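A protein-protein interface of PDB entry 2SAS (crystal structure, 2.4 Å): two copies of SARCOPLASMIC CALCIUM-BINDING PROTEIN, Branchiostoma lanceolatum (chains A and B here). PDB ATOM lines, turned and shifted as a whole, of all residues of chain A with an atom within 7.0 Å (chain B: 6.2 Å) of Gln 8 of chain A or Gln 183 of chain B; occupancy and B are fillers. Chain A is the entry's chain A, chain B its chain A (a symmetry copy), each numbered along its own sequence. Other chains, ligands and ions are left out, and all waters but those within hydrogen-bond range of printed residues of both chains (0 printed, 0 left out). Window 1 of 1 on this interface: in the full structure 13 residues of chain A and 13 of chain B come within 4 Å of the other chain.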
ATOM      1  N   ASN A   3      15.395  -9.292 -21.042  1.00  0.00           N
ATOM      2  CA  ASN A   3      14.244  -9.881 -20.277  1.00  0.00           C
ATOM      3  C   ASN A   3      13.761 -11.055 -21.116  1.00  0.00           C
ATOM      4  O   ASN A   3      14.302 -11.312 -22.231  1.00  0.00           O
ATOM      5  CB  ASN A   3      13.262  -8.783 -19.963  1.00  0.00           C
ATOM      6  CG  ASN A   3      12.675  -8.051 -21.170  1.00  0.00           C
ATOM      7  OD1 ASN A   3      12.731  -8.559 -22.282  1.00  0.00           O
ATOM      8  ND2 ASN A   3      12.099  -6.874 -20.974  1.00  0.00           N
ATOM      9  N   ASP A   4      12.738 -11.722 -20.626  1.00  0.00           N
ATOM     10  CA  ASP A   4      12.123 -12.891 -21.208  1.00  0.00           C
ATOM     11  C   ASP A   4      11.715 -12.595 -22.677  1.00  0.00           C
ATOM     12  O   ASP A   4      12.166 -13.308 -23.562  1.00  0.00           O
ATOM     13  CB  ASP A   4      10.973 -13.438 -20.383  1.00  0.00           C
ATOM     14  CG  ASP A   4      11.372 -14.158 -19.114  1.00  0.00           C
ATOM     15  OD1 ASP A   4      12.550 -14.370 -18.894  1.00  0.00           O
ATOM     16  OD2 ASP A   4      10.497 -14.492 -18.270  1.00  0.00           O
ATOM     17  N   PHE A   5      10.917 -11.569 -22.812  1.00  0.00           N
ATOM     18  CA  PHE A   5      10.380 -11.043 -24.048  1.00  0.00           C
ATOM     19  C   PHE A   5      11.478 -10.860 -25.096  1.00  0.00           C
ATOM     20  O   PHE A   5      11.323 -11.315 -26.238  1.00  0.00           O
ATOM     21  CB  PHE A   5       9.601  -9.733 -23.861  1.00  0.00           C
ATOM     22  CG  PHE A   5       8.994  -9.236 -25.131  1.00  0.00           C
ATOM     23  CD1 PHE A   5       8.073 -10.022 -25.827  1.00  0.00           C
ATOM     24  CD2 PHE A   5       9.388  -7.985 -25.643  1.00  0.00           C
ATOM     25  CE1 PHE A   5       7.539  -9.552 -27.060  1.00  0.00           C
ATOM     26  CE2 PHE A   5       8.830  -7.506 -26.811  1.00  0.00           C
ATOM     27  CZ  PHE A   5       7.889  -8.259 -27.501  1.00  0.00           C
ATOM     28  N   GLN A   6      12.547 -10.175 -24.661  1.00  0.00           N
ATOM     29  CA  GLN A   6      13.666  -9.951 -25.557  1.00  0.00           C
ATOM     30  C   GLN A   6      14.237 -11.270 -26.076  1.00  0.00           C
ATOM     31  O   GLN A   6      14.533 -11.427 -27.257  1.00  0.00           O
ATOM     32  CB  GLN A   6      14.797  -9.129 -24.888  1.00  0.00           C
ATOM     33  CG  GLN A   6      14.364  -7.676 -24.737  1.00  0.00           C
ATOM     34  CD  GLN A   6      15.482  -6.842 -24.144  1.00  0.00           C
ATOM     35  OE1 GLN A   6      15.960  -5.900 -24.764  1.00  0.00           O
ATOM     36  NE2 GLN A   6      15.804  -7.222 -22.890  1.00  0.00           N
ATOM     37  N   LYS A   7      14.427 -12.211 -25.162  1.00  0.00           N
ATOM     38  CA  LYS A   7      15.003 -13.514 -25.426  1.00  0.00           C
ATOM     39  C   LYS A   7      14.124 -14.373 -26.315  1.00  0.00           C
ATOM     40  O   LYS A   7      14.666 -15.217 -27.073  1.00  0.00           O
ATOM     41  CB  LYS A   7      15.405 -14.267 -24.151  1.00  0.00           C
ATOM     42  CG  LYS A   7      16.723 -13.691 -23.619  1.00  0.00           C
ATOM     43  CD  LYS A   7      16.813 -13.703 -22.109  1.00  0.00           C
ATOM     44  CE  LYS A   7      16.505 -15.058 -21.532  1.00  0.00           C
ATOM     45  NZ  LYS A   7      16.356 -14.924 -20.039  1.00  0.00           N
ATOM     46  N   GLN A   8      12.857 -14.130 -26.209  1.00  0.00           N
ATOM     47  CA  GLN A   8      11.821 -14.829 -27.005  1.00  0.00           C
ATOM     48  C   GLN A   8      11.972 -14.471 -28.493  1.00  0.00           C
ATOM     49  O   GLN A   8      11.932 -15.373 -29.364  1.00  0.00           O
ATOM     50  CB  GLN A   8      10.465 -14.445 -26.493  1.00  0.00           C
ATOM     51  CG  GLN A   8       9.240 -15.206 -26.867  1.00  0.00           C
ATOM     52  CD  GLN A   8       7.961 -14.514 -26.374  1.00  0.00           C
ATOM     53  OE1 GLN A   8       7.808 -14.098 -25.217  1.00  0.00           O
ATOM     54  NE2 GLN A   8       7.052 -14.427 -27.348  1.00  0.00           N
ATOM     55  N   LYS A   9      12.134 -13.202 -28.770  1.00  0.00           N
ATOM     56  CA  LYS A   9      12.260 -12.621 -30.109  1.00  0.00           C
ATOM     57  C   LYS A   9      13.629 -12.955 -30.645  1.00  0.00           C
ATOM     58  O   LYS A   9      13.754 -13.127 -31.865  1.00  0.00           O
ATOM     59  CB  LYS A   9      12.008 -11.109 -30.191  1.00  0.00           C
ATOM     60  CG  LYS A   9      10.748 -10.689 -29.406  1.00  0.00           C
ATOM     61  CD  LYS A   9      10.525  -9.200 -29.454  1.00  0.00           C
ATOM     62  CE  LYS A   9      11.771  -8.415 -29.021  1.00  0.00           C
ATOM     63  NZ  LYS A   9      11.543  -6.984 -28.820  1.00  0.00           N
ATOM     64  N   ILE A  10      14.630 -12.989 -29.773  1.00  0.00           N
ATOM     65  CA  ILE A  10      15.974 -13.400 -30.231  1.00  0.00           C
ATOM     66  C   ILE A  10      15.911 -14.871 -30.683  1.00  0.00           C
ATOM     67  O   ILE A  10      16.415 -15.280 -31.736  1.00  0.00           O
ATOM     68  CB  ILE A  10      17.107 -13.055 -29.236  1.00  0.00           C
ATOM     69  CG1 ILE A  10      17.282 -11.489 -29.190  1.00  0.00           C
ATOM     70  CG2 ILE A  10      18.423 -13.656 -29.776  1.00  0.00           C
ATOM     71  CD1 ILE A  10      17.865 -10.912 -27.879  1.00  0.00           C
ATOM     72  N   LYS A  11      15.245 -15.700 -29.918  1.00  0.00           N
ATOM     73  CA  LYS A  11      15.092 -17.116 -30.297  1.00  0.00           C
ATOM     74  C   LYS A  11      14.433 -17.123 -31.684  1.00  0.00           C
ATOM     75  O   LYS A  11      14.903 -17.783 -32.621  1.00  0.00           O
ATOM     76  CB  LYS A  11      14.361 -17.916 -29.260  1.00  0.00           C
ATOM     77  CG  LYS A  11      14.385 -19.451 -29.438  1.00  0.00           C
ATOM     78  CD  LYS A  11      15.803 -19.958 -29.760  1.00  0.00           C
ATOM     79  CE  LYS A  11      15.859 -21.450 -29.513  1.00  0.00           C
ATOM     80  NZ  LYS A  11      15.157 -22.190 -30.613  1.00  0.00           N
ATOM     81  N   PHE A  12      13.355 -16.335 -31.815  1.00  0.00           N
ATOM     82  CA  PHE A  12      12.618 -16.188 -33.054  1.00  0.00           C
ATOM     83  C   PHE A  12      13.525 -15.975 -34.238  1.00  0.00           C
ATOM     84  O   PHE A  12      13.373 -16.719 -35.229  1.00  0.00           O
ATOM     85  CB  PHE A  12      11.520 -15.143 -33.006  1.00  0.00           C
ATOM     86  CG  PHE A  12      10.671 -15.021 -34.235  1.00  0.00           C
ATOM     87  CD1 PHE A  12      11.029 -14.183 -35.275  1.00  0.00           C
ATOM     88  CD2 PHE A  12       9.485 -15.771 -34.319  1.00  0.00           C
ATOM     89  CE1 PHE A  12      10.200 -14.048 -36.401  1.00  0.00           C
ATOM     90  CE2 PHE A  12       8.649 -15.633 -35.436  1.00  0.00           C
ATOM     91  CZ  PHE A  12       9.008 -14.774 -36.469  1.00  0.00           C
ATOM     92  N   THR A  13      14.399 -15.016 -34.224  1.00  0.00           N
ATOM     93  CA  THR A  13      15.336 -14.795 -35.366  1.00  0.00           C
ATOM     94  C   THR A  13      16.323 -15.922 -35.536  1.00  0.00           C
ATOM     95  O   THR A  13      16.804 -16.234 -36.679  1.00  0.00           O
ATOM     96  CB  THR A  13      16.036 -13.398 -35.165  1.00  0.00           C
ATOM     97  OG1 THR A  13      16.948 -13.546 -34.038  1.00  0.00           O
ATOM     98  CG2 THR A  13      15.031 -12.279 -34.860  1.00  0.00           C
ATOM     99  N   TRP A  79      23.165 -21.342 -29.973  1.00  0.00           N
ATOM    100  CA  TRP A  79      22.118 -20.477 -29.409  1.00  0.00           C
ATOM    101  C   TRP A  79      22.720 -19.575 -28.326  1.00  0.00           C
ATOM    102  O   TRP A  79      22.538 -18.357 -28.356  1.00  0.00           O
ATOM    103  CB  TRP A  79      20.997 -21.306 -28.784  1.00  0.00           C
ATOM    104  CG  TRP A  79      20.140 -20.468 -27.875  1.00  0.00           C
ATOM    105  CD1 TRP A  79      19.851 -20.734 -26.572  1.00  0.00           C
ATOM    106  CD2 TRP A  79      19.446 -19.262 -28.214  1.00  0.00           C
ATOM    107  NE1 TRP A  79      18.990 -19.777 -26.083  1.00  0.00           N
ATOM    108  CE2 TRP A  79      18.725 -18.871 -27.068  1.00  0.00           C
ATOM    109  CE3 TRP A  79      19.314 -18.530 -29.397  1.00  0.00           C
ATOM    110  CZ2 TRP A  79      17.878 -17.759 -27.036  1.00  0.00           C
ATOM    111  CZ3 TRP A  79      18.469 -17.412 -29.372  1.00  0.00           C
ATOM    112  CH2 TRP A  79      17.792 -17.029 -28.222  1.00  0.00           C
ATOM    113  N   LEU A 168      12.395  -5.539 -33.376  1.00  0.00           N
ATOM    114  CA  LEU A 168      12.200  -6.969 -33.126  1.00  0.00           C
ATOM    115  C   LEU A 168      13.410  -7.493 -32.316  1.00  0.00           C
ATOM    116  O   LEU A 168      13.297  -8.314 -31.434  1.00  0.00           O
ATOM    117  CB  LEU A 168      12.181  -7.707 -34.491  1.00  0.00           C
ATOM    118  CG  LEU A 168      11.585  -9.078 -34.613  1.00  0.00           C
ATOM    119  CD1 LEU A 168      12.507 -10.034 -35.399  1.00  0.00           C
ATOM    120  CD2 LEU A 168      11.279  -9.732 -33.280  1.00  0.00           C
ATOM    121  N   MET A 181       6.568 -11.107 -36.496  1.00  0.00           N
ATOM    122  CA  MET A 181       6.347 -12.464 -35.942  1.00  0.00           C
ATOM    123  C   MET A 181       4.858 -12.756 -36.220  1.00  0.00           C
ATOM    124  O   MET A 181       4.262 -13.752 -35.824  1.00  0.00           O
ATOM    125  CB  MET A 181       6.712 -12.590 -34.476  1.00  0.00           C
ATOM    126  CG  MET A 181       8.124 -12.342 -34.077  1.00  0.00           C
ATOM    127  SD  MET A 181       8.279 -12.368 -32.228  1.00  0.00           S
ATOM    128  CE  MET A 181       7.371 -10.953 -31.719  1.00  0.00           C
ATOM    129  N   GLN A 183       2.489 -10.671 -35.286  1.00  0.00           N
ATOM    130  CA  GLN A 183       1.530 -10.304 -34.208  1.00  0.00           C
ATOM    131  C   GLN A 183       1.334  -8.841 -33.994  1.00  0.00           C
ATOM    132  O   GLN A 183       2.148  -7.980 -34.338  1.00  0.00           O
ATOM    133  CB  GLN A 183       1.818 -11.125 -32.985  1.00  0.00           C
ATOM    134  CG  GLN A 183       3.216 -11.099 -32.378  1.00  0.00           C
ATOM    135  CD  GLN A 183       2.954 -11.136 -30.865  1.00  0.00           C
ATOM    136  OE1 GLN A 183       2.367 -12.135 -30.454  1.00  0.00           O
ATOM    137  NE2 GLN A 183       3.233 -10.019 -30.219  1.00  0.00           N
ATOM    138  N   PHE B   5      -4.804 -11.140 -27.774  1.00  0.00           N
ATOM    139  CA  PHE B   5      -4.106 -12.210 -27.094  1.00  0.00           C
ATOM    140  C   PHE B   5      -4.867 -13.530 -27.211  1.00  0.00           C
ATOM    141  O   PHE B   5      -4.275 -14.553 -27.582  1.00  0.00           O
ATOM    142  CB  PHE B   5      -3.807 -11.898 -25.621  1.00  0.00           C
ATOM    143  CG  PHE B   5      -3.027 -12.979 -24.949  1.00  0.00           C
ATOM    144  CD1 PHE B   5      -1.766 -13.341 -25.428  1.00  0.00           C
ATOM    145  CD2 PHE B   5      -3.590 -13.658 -23.852  1.00  0.00           C
ATOM    146  CE1 PHE B   5      -1.057 -14.405 -24.804  1.00  0.00           C
ATOM    147  CE2 PHE B   5      -2.880 -14.654 -23.213  1.00  0.00           C
ATOM    148  CZ  PHE B   5      -1.611 -15.007 -23.655  1.00  0.00           C
ATOM    149  N   GLN B   8      -4.912 -14.772 -30.717  1.00  0.00           N
ATOM    150  CA  GLN B   8      -3.541 -15.203 -31.079  1.00  0.00           C
ATOM    151  C   GLN B   8      -3.357 -16.694 -30.751  1.00  0.00           C
ATOM    152  O   GLN B   8      -2.824 -17.461 -31.588  1.00  0.00           O
ATOM    153  CB  GLN B   8      -2.548 -14.361 -30.335  1.00  0.00           C
ATOM    154  CG  GLN B   8      -1.106 -14.332 -30.710  1.00  0.00           C
ATOM    155  CD  GLN B   8      -0.264 -13.549 -29.693  1.00  0.00           C
ATOM    156  OE1 GLN B   8      -0.567 -12.423 -29.273  1.00  0.00           O
ATOM    157  NE2 GLN B   8       0.823 -14.237 -29.334  1.00  0.00           N
ATOM    158  N   PHE B 127       9.490 -32.660 -23.308  1.00  0.00           N
ATOM    159  CA  PHE B 127       9.023 -31.282 -23.502  1.00  0.00           C
ATOM    160  C   PHE B 127       9.913 -30.615 -24.533  1.00  0.00           C
ATOM    161  O   PHE B 127       9.412 -29.963 -25.470  1.00  0.00           O
ATOM    162  CB  PHE B 127       8.854 -30.540 -22.160  1.00  0.00           C
ATOM    163  CG  PHE B 127       8.362 -29.139 -22.400  1.00  0.00           C
ATOM    164  CD1 PHE B 127       7.003 -28.962 -22.741  1.00  0.00           C
ATOM    165  CD2 PHE B 127       9.229 -28.048 -22.358  1.00  0.00           C
ATOM    166  CE1 PHE B 127       6.488 -27.716 -23.055  1.00  0.00           C
ATOM    167  CE2 PHE B 127       8.737 -26.776 -22.630  1.00  0.00           C
ATOM    168  CZ  PHE B 127       7.362 -26.620 -22.997  1.00  0.00           C
ATOM    169  N   GLN B 137       9.413 -21.290 -30.005  1.00  0.00           N
ATOM    170  CA  GLN B 137      10.601 -20.573 -29.555  1.00  0.00           C
ATOM    171  C   GLN B 137      10.958 -20.717 -28.095  1.00  0.00           C
ATOM    172  O   GLN B 137      11.069 -19.732 -27.336  1.00  0.00           O
ATOM    173  CB  GLN B 137      10.625 -19.107 -30.022  1.00  0.00           C
ATOM    174  CG  GLN B 137       9.987 -18.779 -31.363  1.00  0.00           C
ATOM    175  CD  GLN B 137      10.289 -19.720 -32.494  1.00  0.00           C
ATOM    176  OE1 GLN B 137      11.332 -19.697 -33.128  1.00  0.00           O
ATOM    177  NE2 GLN B 137       9.368 -20.638 -32.811  1.00  0.00           N
ATOM    178  N   CYS B 138      11.265 -21.926 -27.659  1.00  0.00           N
ATOM    179  CA  CYS B 138      11.675 -22.218 -26.276  1.00  0.00           C
ATOM    180  C   CYS B 138      13.085 -21.739 -25.987  1.00  0.00           C
ATOM    181  O   CYS B 138      13.997 -22.588 -26.140  1.00  0.00           O
ATOM    182  CB  CYS B 138      11.605 -23.756 -26.167  1.00  0.00           C
ATOM    183  SG  CYS B 138       9.899 -24.350 -26.224  1.00  0.00           S
ATOM    184  N   ALA B 139      13.336 -20.522 -25.556  1.00  0.00           N
ATOM    185  CA  ALA B 139      14.669 -19.981 -25.307  1.00  0.00           C
ATOM    186  C   ALA B 139      15.393 -20.420 -24.044  1.00  0.00           C
ATOM    187  O   ALA B 139      16.618 -20.173 -23.832  1.00  0.00           O
ATOM    188  CB  ALA B 139      14.605 -18.443 -25.308  1.00  0.00           C
ATOM    189  N   VAL B 144      10.896 -22.868 -18.816  1.00  0.00           N
ATOM    190  CA  VAL B 144       9.488 -23.010 -19.254  1.00  0.00           C
ATOM    191  C   VAL B 144       8.958 -24.238 -18.532  1.00  0.00           C
ATOM    192  O   VAL B 144       7.820 -24.292 -18.072  1.00  0.00           O
ATOM    193  CB  VAL B 144       9.364 -23.105 -20.791  1.00  0.00           C
ATOM    194  CG1 VAL B 144       7.990 -23.586 -21.201  1.00  0.00           C
ATOM    195  CG2 VAL B 144       9.747 -21.807 -21.476  1.00  0.00           C
ATOM    196  N   VAL B 147       7.773 -23.463 -14.990  1.00  0.00           N
ATOM    197  CA  VAL B 147       6.461 -22.806 -14.816  1.00  0.00           C
ATOM    198  C   VAL B 147       5.423 -23.931 -14.826  1.00  0.00           C
ATOM    199  O   VAL B 147       4.489 -24.033 -14.028  1.00  0.00           O
ATOM    200  CB  VAL B 147       6.214 -21.759 -15.901  1.00  0.00           C
ATOM    201  CG1 VAL B 147       4.740 -21.312 -15.907  1.00  0.00           C
ATOM    202  CG2 VAL B 147       7.146 -20.578 -15.826  1.00  0.00           C
ATOM    203  N   ALA B 174      -1.855 -13.635 -20.176  1.00  0.00           N
ATOM    204  CA  ALA B 174      -0.702 -14.543 -20.140  1.00  0.00           C
ATOM    205  C   ALA B 174      -0.563 -15.244 -18.807  1.00  0.00           C
ATOM    206  O   ALA B 174      -0.451 -14.617 -17.744  1.00  0.00           O
ATOM    207  CB  ALA B 174       0.556 -13.773 -20.504  1.00  0.00           C
ATOM    208  N   ASP B 175      -0.609 -16.578 -18.855  1.00  0.00           N
ATOM    209  CA  ASP B 175      -0.505 -17.407 -17.631  1.00  0.00           C
ATOM    210  C   ASP B 175       0.217 -18.686 -18.074  1.00  0.00           C
ATOM    211  O   ASP B 175       0.715 -18.759 -19.226  1.00  0.00           O
ATOM    212  CB  ASP B 175      -1.912 -17.590 -17.077  1.00  0.00           C
ATOM    213  CG  ASP B 175      -2.901 -18.380 -17.921  1.00  0.00           C
ATOM    214  OD1 ASP B 175      -2.601 -18.905 -19.002  1.00  0.00           O
ATOM    215  OD2 ASP B 175      -4.065 -18.589 -17.515  1.00  0.00           O
ATOM    216  N   ALA B 176       0.233 -19.663 -17.217  1.00  0.00           N
ATOM    217  CA  ALA B 176       0.862 -20.955 -17.466  1.00  0.00           C
ATOM    218  C   ALA B 176       0.414 -21.632 -18.742  1.00  0.00           C
ATOM    219  O   ALA B 176       1.245 -22.454 -19.244  1.00  0.00           O
ATOM    220  CB  ALA B 176       0.629 -21.932 -16.281  1.00  0.00           C
ATOM    221  N   GLY B 177      -0.802 -21.370 -19.217  1.00  0.00           N
ATOM    222  CA  GLY B 177      -1.281 -22.057 -20.480  1.00  0.00           C
ATOM    223  C   GLY B 177      -0.340 -21.627 -21.589  1.00  0.00           C
ATOM    224  O   GLY B 177      -0.162 -22.266 -22.632  1.00  0.00           O
ATOM    225  N   ASN B 178       0.374 -20.529 -21.433  1.00  0.00           N
ATOM    226  CA  ASN B 178       1.328 -20.084 -22.438  1.00  0.00           C
ATOM    227  C   ASN B 178       2.495 -21.065 -22.687  1.00  0.00           C
ATOM    228  O   ASN B 178       3.112 -20.888 -23.743  1.00  0.00           O
ATOM    229  CB  ASN B 178       1.922 -18.738 -22.137  1.00  0.00           C
ATOM    230  CG  ASN B 178       1.055 -17.507 -22.283  1.00  0.00           C
ATOM    231  OD1 ASN B 178       1.636 -16.440 -22.532  1.00  0.00           O
ATOM    232  ND2 ASN B 178      -0.227 -17.573 -22.082  1.00  0.00           N
ATOM    233  N   THR B 179       2.805 -21.932 -21.781  1.00  0.00           N
ATOM    234  CA  THR B 179       3.912 -22.907 -21.828  1.00  0.00           C
ATOM    235  C   THR B 179       3.808 -23.903 -22.956  1.00  0.00           C
ATOM    236  O   THR B 179       4.843 -24.396 -23.435  1.00  0.00           O
ATOM    237  CB  THR B 179       4.137 -23.613 -20.439  1.00  0.00           C
ATOM    238  OG1 THR B 179       2.951 -24.363 -20.156  1.00  0.00           O
ATOM    239  CG2 THR B 179       4.334 -22.554 -19.318  1.00  0.00           C
ATOM    240  N   LEU B 180       2.566 -24.060 -23.399  1.00  0.00           N
ATOM    241  CA  LEU B 180       2.248 -24.977 -24.498  1.00  0.00           C
ATOM    242  C   LEU B 180       2.661 -24.366 -25.821  1.00  0.00           C
ATOM    243  O   LEU B 180       2.761 -25.061 -26.833  1.00  0.00           O
ATOM    244  CB  LEU B 180       0.809 -25.410 -24.313  1.00  0.00           C
ATOM    245  CG  LEU B 180       0.440 -26.099 -22.997  1.00  0.00           C
ATOM    246  CD1 LEU B 180      -1.045 -26.457 -22.990  1.00  0.00           C
ATOM    247  CD2 LEU B 180       1.254 -27.403 -22.921  1.00  0.00           C
ATOM    248  N   MET B 181       2.942 -23.084 -25.845  1.00  0.00           N
ATOM    249  CA  MET B 181       3.363 -22.405 -27.093  1.00  0.00           C
ATOM    250  C   MET B 181       4.890 -22.241 -26.946  1.00  0.00           C
ATOM    251  O   MET B 181       5.601 -21.633 -27.739  1.00  0.00           O
ATOM    252  CB  MET B 181       2.647 -21.093 -27.344  1.00  0.00           C
ATOM    253  CG  MET B 181       1.170 -21.118 -27.515  1.00  0.00           C
ATOM    254  SD  MET B 181       0.510 -19.386 -27.618  1.00  0.00           S
ATOM    255  CE  MET B 181       0.807 -18.736 -26.013  1.00  0.00           C
ATOM    256  N   GLY B 182       5.334 -22.843 -25.829  1.00  0.00           N
ATOM    257  CA  GLY B 182       6.735 -22.887 -25.460  1.00  0.00           C
ATOM    258  C   GLY B 182       7.167 -21.569 -24.840  1.00  0.00           C
ATOM    259  O   GLY B 182       8.358 -21.240 -24.868  1.00  0.00           O
ATOM    260  N   GLN B 183       6.223 -20.821 -24.293  1.00  0.00           N
ATOM    261  CA  GLN B 183       6.696 -19.546 -23.689  1.00  0.00           C
ATOM    262  C   GLN B 183       6.409 -19.379 -22.234  1.00  0.00           C
ATOM    263  O   GLN B 183       5.522 -19.989 -21.633  1.00  0.00           O
ATOM    264  CB  GLN B 183       6.312 -18.401 -24.580  1.00  0.00           C
ATOM    265  CG  GLN B 183       4.850 -18.208 -24.962  1.00  0.00           C
ATOM    266  CD  GLN B 183       4.670 -16.682 -24.951  1.00  0.00           C
ATOM    267  OE1 GLN B 183       5.370 -16.062 -25.750  1.00  0.00           O
ATOM    268  NE2 GLN B 183       3.922 -16.211 -23.972  1.00  0.00           N
ATOM    269  N   LYS B 184       7.226 -18.527 -21.622  1.00  0.00           N
ATOM    270  CA  LYS B 184       7.021 -18.264 -20.167  1.00  0.00           C
ATOM    271  C   LYS B 184       5.987 -17.146 -20.020  1.00  0.00           C
ATOM    272  O   LYS B 184       6.011 -16.172 -20.780  1.00  0.00           O
ATOM    273  CB  LYS B 184       8.331 -17.726 -19.570  1.00  0.00           C
ATOM    274  CG  LYS B 184       9.291 -18.728 -18.967  1.00  0.00           C
ATOM    275  CD  LYS B 184      10.755 -18.272 -19.093  1.00  0.00           C
ATOM    276  CE  LYS B 184      11.368 -18.863 -20.345  1.00  0.00           C
ATOM    277  NZ  LYS B 184      12.715 -18.323 -20.654  1.00  0.00           N
ATOM    278  N   PRO B 185       5.114 -17.260 -19.022  1.00  0.00           N
ATOM    279  CA  PRO B 185       4.115 -16.220 -18.792  1.00  0.00           C
ATOM    280  C   PRO B 185       4.747 -14.953 -18.244  1.00  0.00           C
ATOM    281  O   PRO B 185       4.974 -14.828 -17.006  1.00  0.00           O
ATOM    282  CB  PRO B 185       3.159 -16.807 -17.772  1.00  0.00           C
ATOM    283  CG  PRO B 185       3.886 -17.898 -17.091  1.00  0.00           C
ATOM    284  CD  PRO B 185       4.905 -18.406 -18.101  1.00  0.00           C
ATOM    285  OXT PRO B 185       4.986 -14.073 -19.027  1.00  0.00           O
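The indole nitrogen of Trp 79 of chain A lies within hydrogen-bond range of the backbone carbonyl oxygen of Ala 139 of chain B, 3.3 Å away. The side-chain amide nitrogen of Gln 8 of chain A sits at hydrogen-bond distance from the side-chain amide oxygen of Gln 183 of chain B (2.8 Å). The side-chain amide oxygen (OE1) of Gln 183 of chain A sits at hydrogen-bond distance from the side-chain amide nitrogen (NE2) of Gln 8 of chain B, at 2.8 Å.
The side-chain amide oxygen of Asn 178 of chain B sits at hydrogen-bond distance from the side-chain amide nitrogen of Gln 183 of chain B (2.7 Å).
Asp 4 of chain A touches Lys 184 of chain B (OD2 to CD, 3.9 Å). O of Lys 7 of chain A touches CB of Ala 139 of chain B, 3.7 Å away. CB of Gln 137 of chain B touches CG of Lys 11 of chain A, at 3.8 Å. Lys 11 of chain A touches Ala 139 of chain B (CB to CB, 3.99 Å). CA of Phe 12 of chain A touches OE1 of Gln 137 of chain B, 3.7 Å away.
Of the printed residues of chain B, Gln 8 of chain A touches Gln 183. Of the printed residues of chain A, Gln 183 of chain B touches Gln 8 (2.8 Å). No residue of chain A comes within 4 Å of Gly 182 of chain B. Printed residues of chain B within 4 Å of Lys 7 of chain A: Ala 139 (3.7 Å). Of the printed residues of chain B, Lys 11 of chain A touches Gln 137 and Ala 139. Met 181 of chain B touches none of the printed residues of chain A. Lys 9 of chain A touches none of the printed residues of chain B. The nearest printed residue of chain B that does not touch Gln 8 of chain A is Gln 137 of chain B (4.01 Å). The nearest residue of chain A that does not touch Gln 183 of chain B is Phe 5 of chain A (6.6 Å). The nearest printed residue of chain A that does not touch Lys 184 of chain B is Lys 7 of chain A (5.0 Å).
Printed residues of chain B that touch a printed residue of chain A: Gln 8, Gln 137, Ala 139, Gln 183 and Lys 184. Hydrophobic or aromatic side chains of chain B within 4 Å of the printed part of chain A: Ala 139. Printed residues of chain A that touch a printed residue of chain B: Asp 4, Lys 7, Gln 8, Lys 11, Phe 12, Trp 79 and Gln 183. Among the printed residues, no Asp or Glu carboxylate lies within 4 Å of a Lys or Arg side-chain nitrogen of the other chain.
Gln 8 of chain A touches Gln 183 of chain B, and with the chains exchanged Gln 183 of chain A touches Gln 8 of chain B. Positions printed for both chains: 5, 8, 181 and 183.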
